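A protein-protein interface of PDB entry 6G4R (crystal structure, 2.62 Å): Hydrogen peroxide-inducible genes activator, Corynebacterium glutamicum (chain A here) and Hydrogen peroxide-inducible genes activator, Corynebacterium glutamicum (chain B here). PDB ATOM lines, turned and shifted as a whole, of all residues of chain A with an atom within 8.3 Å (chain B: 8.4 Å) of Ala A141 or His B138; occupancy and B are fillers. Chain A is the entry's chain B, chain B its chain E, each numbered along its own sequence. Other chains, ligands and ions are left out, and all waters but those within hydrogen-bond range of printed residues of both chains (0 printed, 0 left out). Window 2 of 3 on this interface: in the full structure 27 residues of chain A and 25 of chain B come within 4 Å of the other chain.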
ATOM      1  N   GLN A 135       6.627  13.152  28.918  1.00  0.00           N
ATOM      2  CA  GLN A 135       6.884  12.944  30.334  1.00  0.00           C
ATOM      3  C   GLN A 135       5.600  12.540  31.059  1.00  0.00           C
ATOM      4  O   GLN A 135       4.492  12.614  30.519  1.00  0.00           O
ATOM      5  CB  GLN A 135       7.487  14.203  30.954  1.00  0.00           C
ATOM      6  CG  GLN A 135       8.759  14.664  30.263  1.00  0.00           C
ATOM      7  CD  GLN A 135       9.287  15.972  30.813  1.00  0.00           C
ATOM      8  OE1 GLN A 135       9.043  16.318  31.969  1.00  0.00           O
ATOM      9  NE2 GLN A 135      10.014  16.710  29.983  1.00  0.00           N
ATOM     10  N   THR A 136       5.766  12.110  32.312  1.00  0.00           N
ATOM     11  CA  THR A 136       4.644  11.560  33.067  1.00  0.00           C
ATOM     12  C   THR A 136       3.558  12.605  33.301  1.00  0.00           C
ATOM     13  O   THR A 136       2.364  12.297  33.217  1.00  0.00           O
ATOM     14  CB  THR A 136       5.136  10.990  34.397  1.00  0.00           C
ATOM     15  OG1 THR A 136       6.180  10.039  34.152  1.00  0.00           O
ATOM     16  CG2 THR A 136       4.000  10.295  35.127  1.00  0.00           C
ATOM     17  N   LYS A 137       3.951  13.845  33.602  1.00  0.00           N
ATOM     18  CA  LYS A 137       2.960  14.879  33.891  1.00  0.00           C
ATOM     19  C   LYS A 137       2.110  15.183  32.664  1.00  0.00           C
ATOM     20  O   LYS A 137       0.888  15.339  32.768  1.00  0.00           O
ATOM     21  CB  LYS A 137       3.648  16.152  34.380  1.00  0.00           C
ATOM     22  CG  LYS A 137       2.679  17.215  34.874  1.00  0.00           C
ATOM     23  CD  LYS A 137       3.400  18.496  35.259  1.00  0.00           C
ATOM     24  CE  LYS A 137       3.711  19.331  34.025  1.00  0.00           C
ATOM     25  NZ  LYS A 137       4.426  20.592  34.365  1.00  0.00           N
ATOM     26  N   HIS A 138       2.740  15.274  31.491  1.00  0.00           N
ATOM     27  CA  HIS A 138       1.989  15.567  30.276  1.00  0.00           C
ATOM     28  C   HIS A 138       1.113  14.394  29.856  1.00  0.00           C
ATOM     29  O   HIS A 138       0.043  14.603  29.276  1.00  0.00           O
ATOM     30  CB  HIS A 138       2.946  15.953  29.150  1.00  0.00           C
ATOM     31  CG  HIS A 138       3.832  17.114  29.481  1.00  0.00           C
ATOM     32  ND1 HIS A 138       5.091  16.959  30.021  1.00  0.00           N
ATOM     33  CD2 HIS A 138       3.640  18.448  29.351  1.00  0.00           C
ATOM     34  CE1 HIS A 138       5.636  18.148  30.208  1.00  0.00           C
ATOM     35  NE2 HIS A 138       4.777  19.069  29.810  1.00  0.00           N
ATOM     36  N   LEU A 139       1.539  13.161  30.145  1.00  0.00           N
ATOM     37  CA  LEU A 139       0.720  12.000  29.812  1.00  0.00           C
ATOM     38  C   LEU A 139      -0.573  11.986  30.618  1.00  0.00           C
ATOM     39  O   LEU A 139      -1.659  11.775  30.065  1.00  0.00           O
ATOM     40  CB  LEU A 139       1.510  10.711  30.045  1.00  0.00           C
ATOM     41  CG  LEU A 139       2.632  10.394  29.055  1.00  0.00           C
ATOM     42  CD1 LEU A 139       3.172   8.994  29.298  1.00  0.00           C
ATOM     43  CD2 LEU A 139       2.146  10.545  27.622  1.00  0.00           C
ATOM     44  N   LEU A 140      -0.476  12.204  31.932  1.00  0.00           N
ATOM     45  CA  LEU A 140      -1.675  12.247  32.762  1.00  0.00           C
ATOM     46  C   LEU A 140      -2.577  13.412  32.379  1.00  0.00           C
ATOM     47  O   LEU A 140      -3.805  13.296  32.451  1.00  0.00           O
ATOM     48  CB  LEU A 140      -1.287  12.330  34.240  1.00  0.00           C
ATOM     49  CG  LEU A 140      -0.644  11.072  34.826  1.00  0.00           C
ATOM     50  CD1 LEU A 140      -0.127  11.331  36.232  1.00  0.00           C
ATOM     51  CD2 LEU A 140      -1.631   9.913  34.819  1.00  0.00           C
ATOM     52  N   ALA A 141      -1.989  14.539  31.976  1.00  0.00           N
ATOM     53  CA  ALA A 141      -2.784  15.658  31.480  1.00  0.00           C
ATOM     54  C   ALA A 141      -3.530  15.275  30.208  1.00  0.00           C
ATOM     55  O   ALA A 141      -4.738  15.509  30.087  1.00  0.00           O
ATOM     56  CB  ALA A 141      -1.889  16.874  31.242  1.00  0.00           C
ATOM     57  N   LEU A 142      -2.820  14.688  29.241  1.00  0.00           N
ATOM     58  CA  LEU A 142      -3.466  14.229  28.016  1.00  0.00           C
ATOM     59  C   LEU A 142      -4.459  13.104  28.274  1.00  0.00           C
ATOM     60  O   LEU A 142      -5.364  12.894  27.460  1.00  0.00           O
ATOM     61  CB  LEU A 142      -2.415  13.763  27.006  1.00  0.00           C
ATOM     62  CG  LEU A 142      -1.435  14.809  26.468  1.00  0.00           C
ATOM     63  CD1 LEU A 142      -0.416  14.160  25.541  1.00  0.00           C
ATOM     64  CD2 LEU A 142      -2.171  15.936  25.760  1.00  0.00           C
ATOM     65  N   LEU A 143      -4.316  12.380  29.386  1.00  0.00           N
ATOM     66  CA  LEU A 143      -5.234  11.288  29.685  1.00  0.00           C
ATOM     67  C   LEU A 143      -6.551  11.803  30.258  1.00  0.00           C
ATOM     68  O   LEU A 143      -7.620  11.276  29.927  1.00  0.00           O
ATOM     69  CB  LEU A 143      -4.574  10.299  30.647  1.00  0.00           C
ATOM     70  CG  LEU A 143      -5.256   8.940  30.819  1.00  0.00           C
ATOM     71  CD1 LEU A 143      -5.436   8.255  29.474  1.00  0.00           C
ATOM     72  CD2 LEU A 143      -4.456   8.055  31.764  1.00  0.00           C
ATOM     73  N   ARG A 144      -6.497  12.826  31.114  1.00  0.00           N
ATOM     74  CA  ARG A 144      -7.726  13.425  31.626  1.00  0.00           C
ATOM     75  C   ARG A 144      -8.518  14.103  30.516  1.00  0.00           C
ATOM     76  O   ARG A 144      -9.748  13.994  30.466  1.00  0.00           O
ATOM     77  CB  ARG A 144      -7.406  14.426  32.735  1.00  0.00           C
ATOM     78  CG  ARG A 144      -7.204  13.805  34.105  1.00  0.00           C
ATOM     79  CD  ARG A 144      -7.042  14.877  35.169  1.00  0.00           C
ATOM     80  NE  ARG A 144      -5.841  15.679  34.955  1.00  0.00           N
ATOM     81  CZ  ARG A 144      -4.646  15.383  35.455  1.00  0.00           C
ATOM     82  NH1 ARG A 144      -4.488  14.299  36.202  1.00  0.00           N
ATOM     83  NH2 ARG A 144      -3.608  16.171  35.207  1.00  0.00           N
ATOM     84  N   ASP A 145      -7.832  14.807  29.618  1.00  0.00           N
ATOM     85  CA  ASP A 145      -8.480  15.533  28.533  1.00  0.00           C
ATOM     86  C   ASP A 145      -8.783  14.654  27.324  1.00  0.00           C
ATOM     87  O   ASP A 145      -9.158  15.185  26.273  1.00  0.00           O
ATOM     88  CB  ASP A 145      -7.614  16.724  28.113  1.00  0.00           C
ATOM     89  CG  ASP A 145      -7.505  17.775  29.202  1.00  0.00           C
ATOM     90  OD1 ASP A 145      -8.546  18.128  29.793  1.00  0.00           O
ATOM     91  OD2 ASP A 145      -6.379  18.243  29.472  1.00  0.00           O
ATOM     92  N   GLY A 146      -8.624  13.338  27.444  1.00  0.00           N
ATOM     93  CA  GLY A 146      -8.993  12.421  26.386  1.00  0.00           C
ATOM     94  C   GLY A 146      -8.064  12.379  25.195  1.00  0.00           C
ATOM     95  O   GLY A 146      -8.381  11.704  24.209  1.00  0.00           O
ATOM     96  N   ALA A 147      -6.925  13.075  25.246  1.00  0.00           N
ATOM     97  CA  ALA A 147      -6.039  13.118  24.086  1.00  0.00           C
ATOM     98  C   ALA A 147      -5.364  11.775  23.845  1.00  0.00           C
ATOM     99  O   ALA A 147      -4.976  11.473  22.711  1.00  0.00           O
ATOM    100  CB  ALA A 147      -4.992  14.217  24.261  1.00  0.00           C
ATOM    101  N   ILE A 148      -5.212  10.962  24.889  1.00  0.00           N
ATOM    102  CA  ILE A 148      -4.720   9.598  24.764  1.00  0.00           C
ATOM    103  C   ILE A 148      -5.675   8.690  25.524  1.00  0.00           C
ATOM    104  O   ILE A 148      -6.360   9.118  26.457  1.00  0.00           O
ATOM    105  CB  ILE A 148      -3.273   9.434  25.284  1.00  0.00           C
ATOM    106  CG1 ILE A 148      -3.217   9.595  26.803  1.00  0.00           C
ATOM    107  CG2 ILE A 148      -2.339  10.425  24.605  1.00  0.00           C
ATOM    108  CD1 ILE A 148      -1.829   9.424  27.381  1.00  0.00           C
ATOM    109  N   ALA A 151      -2.027   5.050  29.194  1.00  0.00           N
ATOM    110  CA  ALA A 151      -0.671   5.527  29.419  1.00  0.00           C
ATOM    111  C   ALA A 151       0.162   4.457  30.107  1.00  0.00           C
ATOM    112  O   ALA A 151      -0.287   3.826  31.069  1.00  0.00           O
ATOM    113  CB  ALA A 151      -0.669   6.807  30.263  1.00  0.00           C
ATOM    114  N   MET A 153       3.419   3.994  32.303  1.00  0.00           N
ATOM    115  CA  MET A 153       4.256   4.817  33.167  1.00  0.00           C
ATOM    116  C   MET A 153       4.578   4.033  34.433  1.00  0.00           C
ATOM    117  O   MET A 153       4.144   2.892  34.613  1.00  0.00           O
ATOM    118  CB  MET A 153       3.569   6.146  33.492  1.00  0.00           C
ATOM    119  CG  MET A 153       2.241   5.990  34.211  1.00  0.00           C
ATOM    120  SD  MET A 153       1.507   7.572  34.660  1.00  0.00           S
ATOM    121  CE  MET A 153       1.264   8.303  33.044  1.00  0.00           C
ATOM    122  N   ALA A 159      -2.476   9.726  40.677  1.00  0.00           N
ATOM    123  CA  ALA A 159      -3.479  10.614  40.106  1.00  0.00           C
ATOM    124  C   ALA A 159      -4.883  10.097  40.407  1.00  0.00           C
ATOM    125  O   ALA A 159      -5.147   8.899  40.265  1.00  0.00           O
ATOM    126  CB  ALA A 159      -3.295  10.739  38.596  1.00  0.00           C
ATOM    127  N   MET A 162      -8.104   7.820  38.107  1.00  0.00           N
ATOM    128  CA  MET A 162      -7.429   6.897  37.210  1.00  0.00           C
ATOM    129  C   MET A 162      -7.334   5.526  37.867  1.00  0.00           C
ATOM    130  O   MET A 162      -7.365   5.399  39.094  1.00  0.00           O
ATOM    131  CB  MET A 162      -6.028   7.409  36.857  1.00  0.00           C
ATOM    132  CG  MET A 162      -5.973   8.902  36.562  1.00  0.00           C
ATOM    133  SD  MET A 162      -7.036   9.419  35.204  1.00  0.00           S
ATOM    134  CE  MET A 162      -5.869  10.328  34.195  1.00  0.00           C
ATOM    135  N   ARG A 285      -8.535   5.849  32.472  1.00  0.00           N
ATOM    136  CA  ARG A 285      -9.558   6.593  33.193  1.00  0.00           C
ATOM    137  C   ARG A 285     -10.535   5.652  33.891  1.00  0.00           C
ATOM    138  O   ARG A 285     -10.861   4.572  33.392  1.00  0.00           O
ATOM    139  CB  ARG A 285     -10.317   7.518  32.241  1.00  0.00           C
ATOM    140  CG  ARG A 285      -9.457   8.594  31.599  1.00  0.00           C
ATOM    141  CD  ARG A 285     -10.266   9.446  30.635  1.00  0.00           C
ATOM    142  NE  ARG A 285     -10.608   8.720  29.416  1.00  0.00           N
ATOM    143  CZ  ARG A 285      -9.888   8.753  28.300  1.00  0.00           C
ATOM    144  NH1 ARG A 285      -8.783   9.483  28.243  1.00  0.00           N
ATOM    145  NH2 ARG A 285     -10.275   8.060  27.237  1.00  0.00           N
ATOM    146  N   GLY B 103      -9.856  26.478  24.899  1.00  0.00           N
ATOM    147  CA  GLY B 103      -8.850  26.443  25.945  1.00  0.00           C
ATOM    148  C   GLY B 103      -8.435  27.855  26.321  1.00  0.00           C
ATOM    149  O   GLY B 103      -8.189  28.693  25.453  1.00  0.00           O
ATOM    150  N   VAL B 132     -11.685  24.606  28.777  1.00  0.00           N
ATOM    151  CA  VAL B 132     -10.543  23.853  29.284  1.00  0.00           C
ATOM    152  C   VAL B 132      -9.515  24.862  29.776  1.00  0.00           C
ATOM    153  O   VAL B 132      -8.945  25.617  28.978  1.00  0.00           O
ATOM    154  CB  VAL B 132      -9.941  22.926  28.219  1.00  0.00           C
ATOM    155  CG1 VAL B 132      -8.649  22.305  28.726  1.00  0.00           C
ATOM    156  CG2 VAL B 132     -10.939  21.847  27.831  1.00  0.00           C
ATOM    157  N   GLU B 133      -9.279  24.885  31.084  1.00  0.00           N
ATOM    158  CA  GLU B 133      -8.319  25.800  31.689  1.00  0.00           C
ATOM    159  C   GLU B 133      -7.044  25.040  32.029  1.00  0.00           C
ATOM    160  O   GLU B 133      -7.060  24.139  32.874  1.00  0.00           O
ATOM    161  CB  GLU B 133      -8.890  26.452  32.947  1.00  0.00           C
ATOM    162  CG  GLU B 133      -7.938  27.449  33.591  1.00  0.00           C
ATOM    163  CD  GLU B 133      -8.314  27.781  35.019  1.00  0.00           C
ATOM    164  OE1 GLU B 133      -8.819  26.882  35.723  1.00  0.00           O
ATOM    165  OE2 GLU B 133      -8.105  28.939  35.437  1.00  0.00           O
ATOM    166  N   ASP B 134      -5.948  25.407  31.374  1.00  0.00           N
ATOM    167  CA  ASP B 134      -4.642  24.830  31.662  1.00  0.00           C
ATOM    168  C   ASP B 134      -3.577  25.780  31.129  1.00  0.00           C
ATOM    169  O   ASP B 134      -3.882  26.802  30.509  1.00  0.00           O
ATOM    170  CB  ASP B 134      -4.510  23.427  31.062  1.00  0.00           C
ATOM    171  CG  ASP B 134      -3.791  22.464  31.988  1.00  0.00           C
ATOM    172  OD1 ASP B 134      -2.698  22.817  32.480  1.00  0.00           O
ATOM    173  OD2 ASP B 134      -4.322  21.359  32.227  1.00  0.00           O
ATOM    174  N   GLN B 135      -2.317  25.430  31.373  1.00  0.00           N
ATOM    175  CA  GLN B 135      -1.210  26.291  30.994  1.00  0.00           C
ATOM    176  C   GLN B 135      -0.979  26.242  29.484  1.00  0.00           C
ATOM    177  O   GLN B 135      -1.575  25.442  28.759  1.00  0.00           O
ATOM    178  CB  GLN B 135       0.052  25.896  31.760  1.00  0.00           C
ATOM    179  CG  GLN B 135      -0.119  25.973  33.269  1.00  0.00           C
ATOM    180  CD  GLN B 135       1.131  25.576  34.024  1.00  0.00           C
ATOM    181  OE1 GLN B 135       2.240  25.651  33.495  1.00  0.00           O
ATOM    182  NE2 GLN B 135       0.959  25.148  35.269  1.00  0.00           N
ATOM    183  N   THR B 136      -0.087  27.120  29.017  1.00  0.00           N
ATOM    184  CA  THR B 136       0.052  27.354  27.581  1.00  0.00           C
ATOM    185  C   THR B 136       0.550  26.113  26.849  1.00  0.00           C
ATOM    186  O   THR B 136       0.082  25.809  25.745  1.00  0.00           O
ATOM    187  CB  THR B 136       0.992  28.534  27.332  1.00  0.00           C
ATOM    188  OG1 THR B 136       0.520  29.681  28.049  1.00  0.00           O
ATOM    189  CG2 THR B 136       1.051  28.866  25.847  1.00  0.00           C
ATOM    190  N   LYS B 137       1.502  25.386  27.439  1.00  0.00           N
ATOM    191  CA  LYS B 137       2.062  24.224  26.755  1.00  0.00           C
ATOM    192  C   LYS B 137       1.017  23.134  26.555  1.00  0.00           C
ATOM    193  O   LYS B 137       0.942  22.530  25.478  1.00  0.00           O
ATOM    194  CB  LYS B 137       3.249  23.665  27.537  1.00  0.00           C
ATOM    195  CG  LYS B 137       3.975  22.546  26.805  1.00  0.00           C
ATOM    196  CD  LYS B 137       5.096  21.951  27.640  1.00  0.00           C
ATOM    197  CE  LYS B 137       5.912  20.957  26.827  1.00  0.00           C
ATOM    198  NZ  LYS B 137       7.112  20.475  27.566  1.00  0.00           N
ATOM    199  N   HIS B 138       0.202  22.864  27.577  1.00  0.00           N
ATOM    200  CA  HIS B 138      -0.813  21.827  27.443  1.00  0.00           C
ATOM    201  C   HIS B 138      -1.928  22.252  26.497  1.00  0.00           C
ATOM    202  O   HIS B 138      -2.531  21.403  25.831  1.00  0.00           O
ATOM    203  CB  HIS B 138      -1.381  21.458  28.811  1.00  0.00           C
ATOM    204  CG  HIS B 138      -2.349  20.317  28.774  1.00  0.00           C
ATOM    205  ND1 HIS B 138      -2.038  19.097  28.211  1.00  0.00           N
ATOM    206  CD2 HIS B 138      -3.619  20.208  29.228  1.00  0.00           C
ATOM    207  CE1 HIS B 138      -3.076  18.287  28.318  1.00  0.00           C
ATOM    208  NE2 HIS B 138      -4.048  18.936  28.933  1.00  0.00           N
ATOM    209  N   LEU B 139      -2.219  23.554  26.424  1.00  0.00           N
ATOM    210  CA  LEU B 139      -3.233  24.033  25.490  1.00  0.00           C
ATOM    211  C   LEU B 139      -2.795  23.805  24.048  1.00  0.00           C
ATOM    212  O   LEU B 139      -3.573  23.315  23.221  1.00  0.00           O
ATOM    213  CB  LEU B 139      -3.521  25.513  25.740  1.00  0.00           C
ATOM    214  CG  LEU B 139      -4.292  25.851  27.019  1.00  0.00           C
ATOM    215  CD1 LEU B 139      -4.689  27.319  27.033  1.00  0.00           C
ATOM    216  CD2 LEU B 139      -5.514  24.957  27.169  1.00  0.00           C
ATOM    217  N   LEU B 140      -1.549  24.163  23.728  1.00  0.00           N
ATOM    218  CA  LEU B 140      -1.030  23.915  22.388  1.00  0.00           C
ATOM    219  C   LEU B 140      -0.949  22.424  22.093  1.00  0.00           C
ATOM    220  O   LEU B 140      -1.151  22.007  20.946  1.00  0.00           O
ATOM    221  CB  LEU B 140       0.343  24.568  22.226  1.00  0.00           C
ATOM    222  CG  LEU B 140       0.349  26.098  22.190  1.00  0.00           C
ATOM    223  CD1 LEU B 140       1.772  26.633  22.223  1.00  0.00           C
ATOM    224  CD2 LEU B 140      -0.390  26.606  20.962  1.00  0.00           C
ATOM    225  N   ALA B 141      -0.651  21.609  23.107  1.00  0.00           N
ATOM    226  CA  ALA B 141      -0.675  20.161  22.929  1.00  0.00           C
ATOM    227  C   ALA B 141      -2.079  19.684  22.580  1.00  0.00           C
ATOM    228  O   ALA B 141      -2.271  18.925  21.623  1.00  0.00           O
ATOM    229  CB  ALA B 141      -0.162  19.466  24.189  1.00  0.00           C
ATOM    230  N   LEU B 142      -3.077  20.118  23.354  1.00  0.00           N
ATOM    231  CA  LEU B 142      -4.460  19.783  23.040  1.00  0.00           C
ATOM    232  C   LEU B 142      -4.915  20.401  21.725  1.00  0.00           C
ATOM    233  O   LEU B 142      -5.873  19.907  21.123  1.00  0.00           O
ATOM    234  CB  LEU B 142      -5.390  20.234  24.167  1.00  0.00           C
ATOM    235  CG  LEU B 142      -5.218  19.573  25.536  1.00  0.00           C
ATOM    236  CD1 LEU B 142      -6.171  20.189  26.550  1.00  0.00           C
ATOM    237  CD2 LEU B 142      -5.424  18.070  25.443  1.00  0.00           C
ATOM    238  N   LEU B 143      -4.258  21.473  21.274  1.00  0.00           N
ATOM    239  CA  LEU B 143      -4.641  22.098  20.013  1.00  0.00           C
ATOM    240  C   LEU B 143      -4.076  21.346  18.813  1.00  0.00           C
ATOM    241  O   LEU B 143      -4.754  21.218  17.789  1.00  0.00           O
ATOM    242  CB  LEU B 143      -4.190  23.555  19.983  1.00  0.00           C
ATOM    243  CG  LEU B 143      -4.841  24.353  18.856  1.00  0.00           C
ATOM    244  CD1 LEU B 143      -6.358  24.269  18.948  1.00  0.00           C
ATOM    245  CD2 LEU B 143      -4.383  25.785  18.893  1.00  0.00           C
ATOM    246  N   ARG B 144      -2.834  20.859  18.910  1.00  0.00           N
ATOM    247  CA  ARG B 144      -2.296  20.028  17.837  1.00  0.00           C
ATOM    248  C   ARG B 144      -3.079  18.729  17.725  1.00  0.00           C
ATOM    249  O   ARG B 144      -3.417  18.288  16.620  1.00  0.00           O
ATOM    250  CB  ARG B 144      -0.812  19.747  18.072  1.00  0.00           C
ATOM    251  CG  ARG B 144       0.114  20.847  17.582  1.00  0.00           C
ATOM    252  CD  ARG B 144       1.576  20.451  17.713  1.00  0.00           C
ATOM    253  NE  ARG B 144       1.970  20.273  19.107  1.00  0.00           N
ATOM    254  CZ  ARG B 144       2.449  21.246  19.876  1.00  0.00           C
ATOM    255  NH1 ARG B 144       2.595  22.471  19.386  1.00  0.00           N
ATOM    256  NH2 ARG B 144       2.784  20.997  21.134  1.00  0.00           N
ATOM    257  N   ASP B 145      -3.383  18.109  18.861  1.00  0.00           N
ATOM    258  CA  ASP B 145      -4.373  17.049  18.893  1.00  0.00           C
ATOM    259  C   ASP B 145      -5.762  17.641  18.649  1.00  0.00           C
ATOM    260  O   ASP B 145      -5.948  18.858  18.581  1.00  0.00           O
ATOM    261  CB  ASP B 145      -4.324  16.317  20.235  1.00  0.00           C
ATOM    262  CG  ASP B 145      -4.803  14.882  20.139  1.00  0.00           C
ATOM    263  OD1 ASP B 145      -3.965  13.990  19.889  1.00  0.00           O
ATOM    264  OD2 ASP B 145      -6.018  14.647  20.309  1.00  0.00           O
ATOM    265  N   ALA B 147      -8.286  17.522  20.703  1.00  0.00           N
ATOM    266  CA  ALA B 147      -9.038  17.658  21.950  1.00  0.00           C
ATOM    267  C   ALA B 147      -9.644  19.046  22.139  1.00  0.00           C
ATOM    268  O   ALA B 147     -10.652  19.177  22.844  1.00  0.00           O
ATOM    269  CB  ALA B 147      -8.139  17.314  23.136  1.00  0.00           C
ATOM    270  N   ILE B 148      -9.060  20.091  21.556  1.00  0.00           N
ATOM    271  CA  ILE B 148      -9.673  21.415  21.604  1.00  0.00           C
ATOM    272  C   ILE B 148      -9.676  22.027  20.212  1.00  0.00           C
ATOM    273  O   ILE B 148      -8.834  21.708  19.365  1.00  0.00           O
ATOM    274  CB  ILE B 148      -8.973  22.367  22.606  1.00  0.00           C
ATOM    275  CG1 ILE B 148      -7.577  22.747  22.117  1.00  0.00           C
ATOM    276  CG2 ILE B 148      -8.915  21.752  24.000  1.00  0.00           C
ATOM    277  CD1 ILE B 148      -6.852  23.698  23.045  1.00  0.00           C
ATOM    278  N   ALA B 151      -7.785  28.098  21.177  1.00  0.00           N
ATOM    279  CA  ALA B 151      -7.120  28.409  22.434  1.00  0.00           C
ATOM    280  C   ALA B 151      -6.949  29.912  22.588  1.00  0.00           C
ATOM    281  O   ALA B 151      -6.553  30.603  21.645  1.00  0.00           O
ATOM    282  CB  ALA B 151      -5.753  27.719  22.524  1.00  0.00           C
ATOM    283  N   MET B 153      -4.762  32.625  24.481  1.00  0.00           N
ATOM    284  CA  MET B 153      -3.466  32.701  25.143  1.00  0.00           C
ATOM    285  C   MET B 153      -2.780  33.992  24.717  1.00  0.00           C
ATOM    286  O   MET B 153      -3.309  34.768  23.917  1.00  0.00           O
ATOM    287  CB  MET B 153      -2.612  31.472  24.818  1.00  0.00           C
ATOM    288  CG  MET B 153      -2.320  31.296  23.338  1.00  0.00           C
ATOM    289  SD  MET B 153      -1.250  29.885  23.003  1.00  0.00           S
ATOM    290  CE  MET B 153      -2.273  28.540  23.594  1.00  0.00           C
ATOM    291  N   GLY B 204       5.847  27.731  34.137  1.00  0.00           N
ATOM    292  CA  GLY B 204       4.946  27.378  33.060  1.00  0.00           C
ATOM    293  C   GLY B 204       3.887  28.406  32.743  1.00  0.00           C
ATOM    294  O   GLY B 204       3.173  28.262  31.748  1.00  0.00           O
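A ring nitrogen (NE2) of His B138 lies within hydrogen-bond range of the side-chain carboxylate of Asp A145.
O of Leu A142 sits at hydrogen-bond distance from N of Ile A148, at 3.2 Å. The backbone carbonyl oxygen (O) of Leu B142 lies within hydrogen-bond range of the backbone NH (N) of Ile B148 (3.2 Å). The backbone carbonyl oxygen (O) of Leu B142 is in hydrogen-bond range of the backbone NH (N) of Ala B147, 3.4 Å away. O of Leu A142 is in hydrogen-bond range of N of Ala A147, at 2.7 Å.
Among the printed residues, merely in contact across the chains: His A138 with Lys B137 (3.5 Å), Ala A141 with His B138 (3.5 Å), Leu A142 with His B138 (3.6 Å), Leu A142 with Leu B142 (3.9 Å), Asp A145 with Leu B142 (3.5 Å), Asp A145 with Ala B147 (3.9 Å) and Ala A147 with Asp B145 (3.9 Å).
Of chain B, only His B138 (3.5 Å) comes within 4 Å of Ala A141. Of chain A, only Ala A141, Leu A142 and Asp A145 come within 4 Å of His B138. Of the printed residues of chain B, His A138 touches Lys B137. Printed residues of chain B within 4 Å of Leu A142: His B138 and Leu B142. Of the printed residues of chain A, Leu B142 touches Leu A142 (3.9 Å) and Asp A145 (3.5 Å). Printed residues of chain B within 4 Å of Ala A147: Asp B145 (3.9 Å). Of the printed residues of chain A, Asp B145 touches Ala A147. The nearest residue of chain B that does not touch Ala A141 is Asp B134 (5.2 Å).
Of the 20 printed residues of chain B, 5 touch a printed residue of chain A. Of the 19 printed residues of chain A, 5 touch a printed residue of chain B. Hydrophobic or aromatic side chains of chain A that line the printed part of chain B: His A138, Ala A141 and Leu A142. Among the printed residues, 8 pairs touch across the chains.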
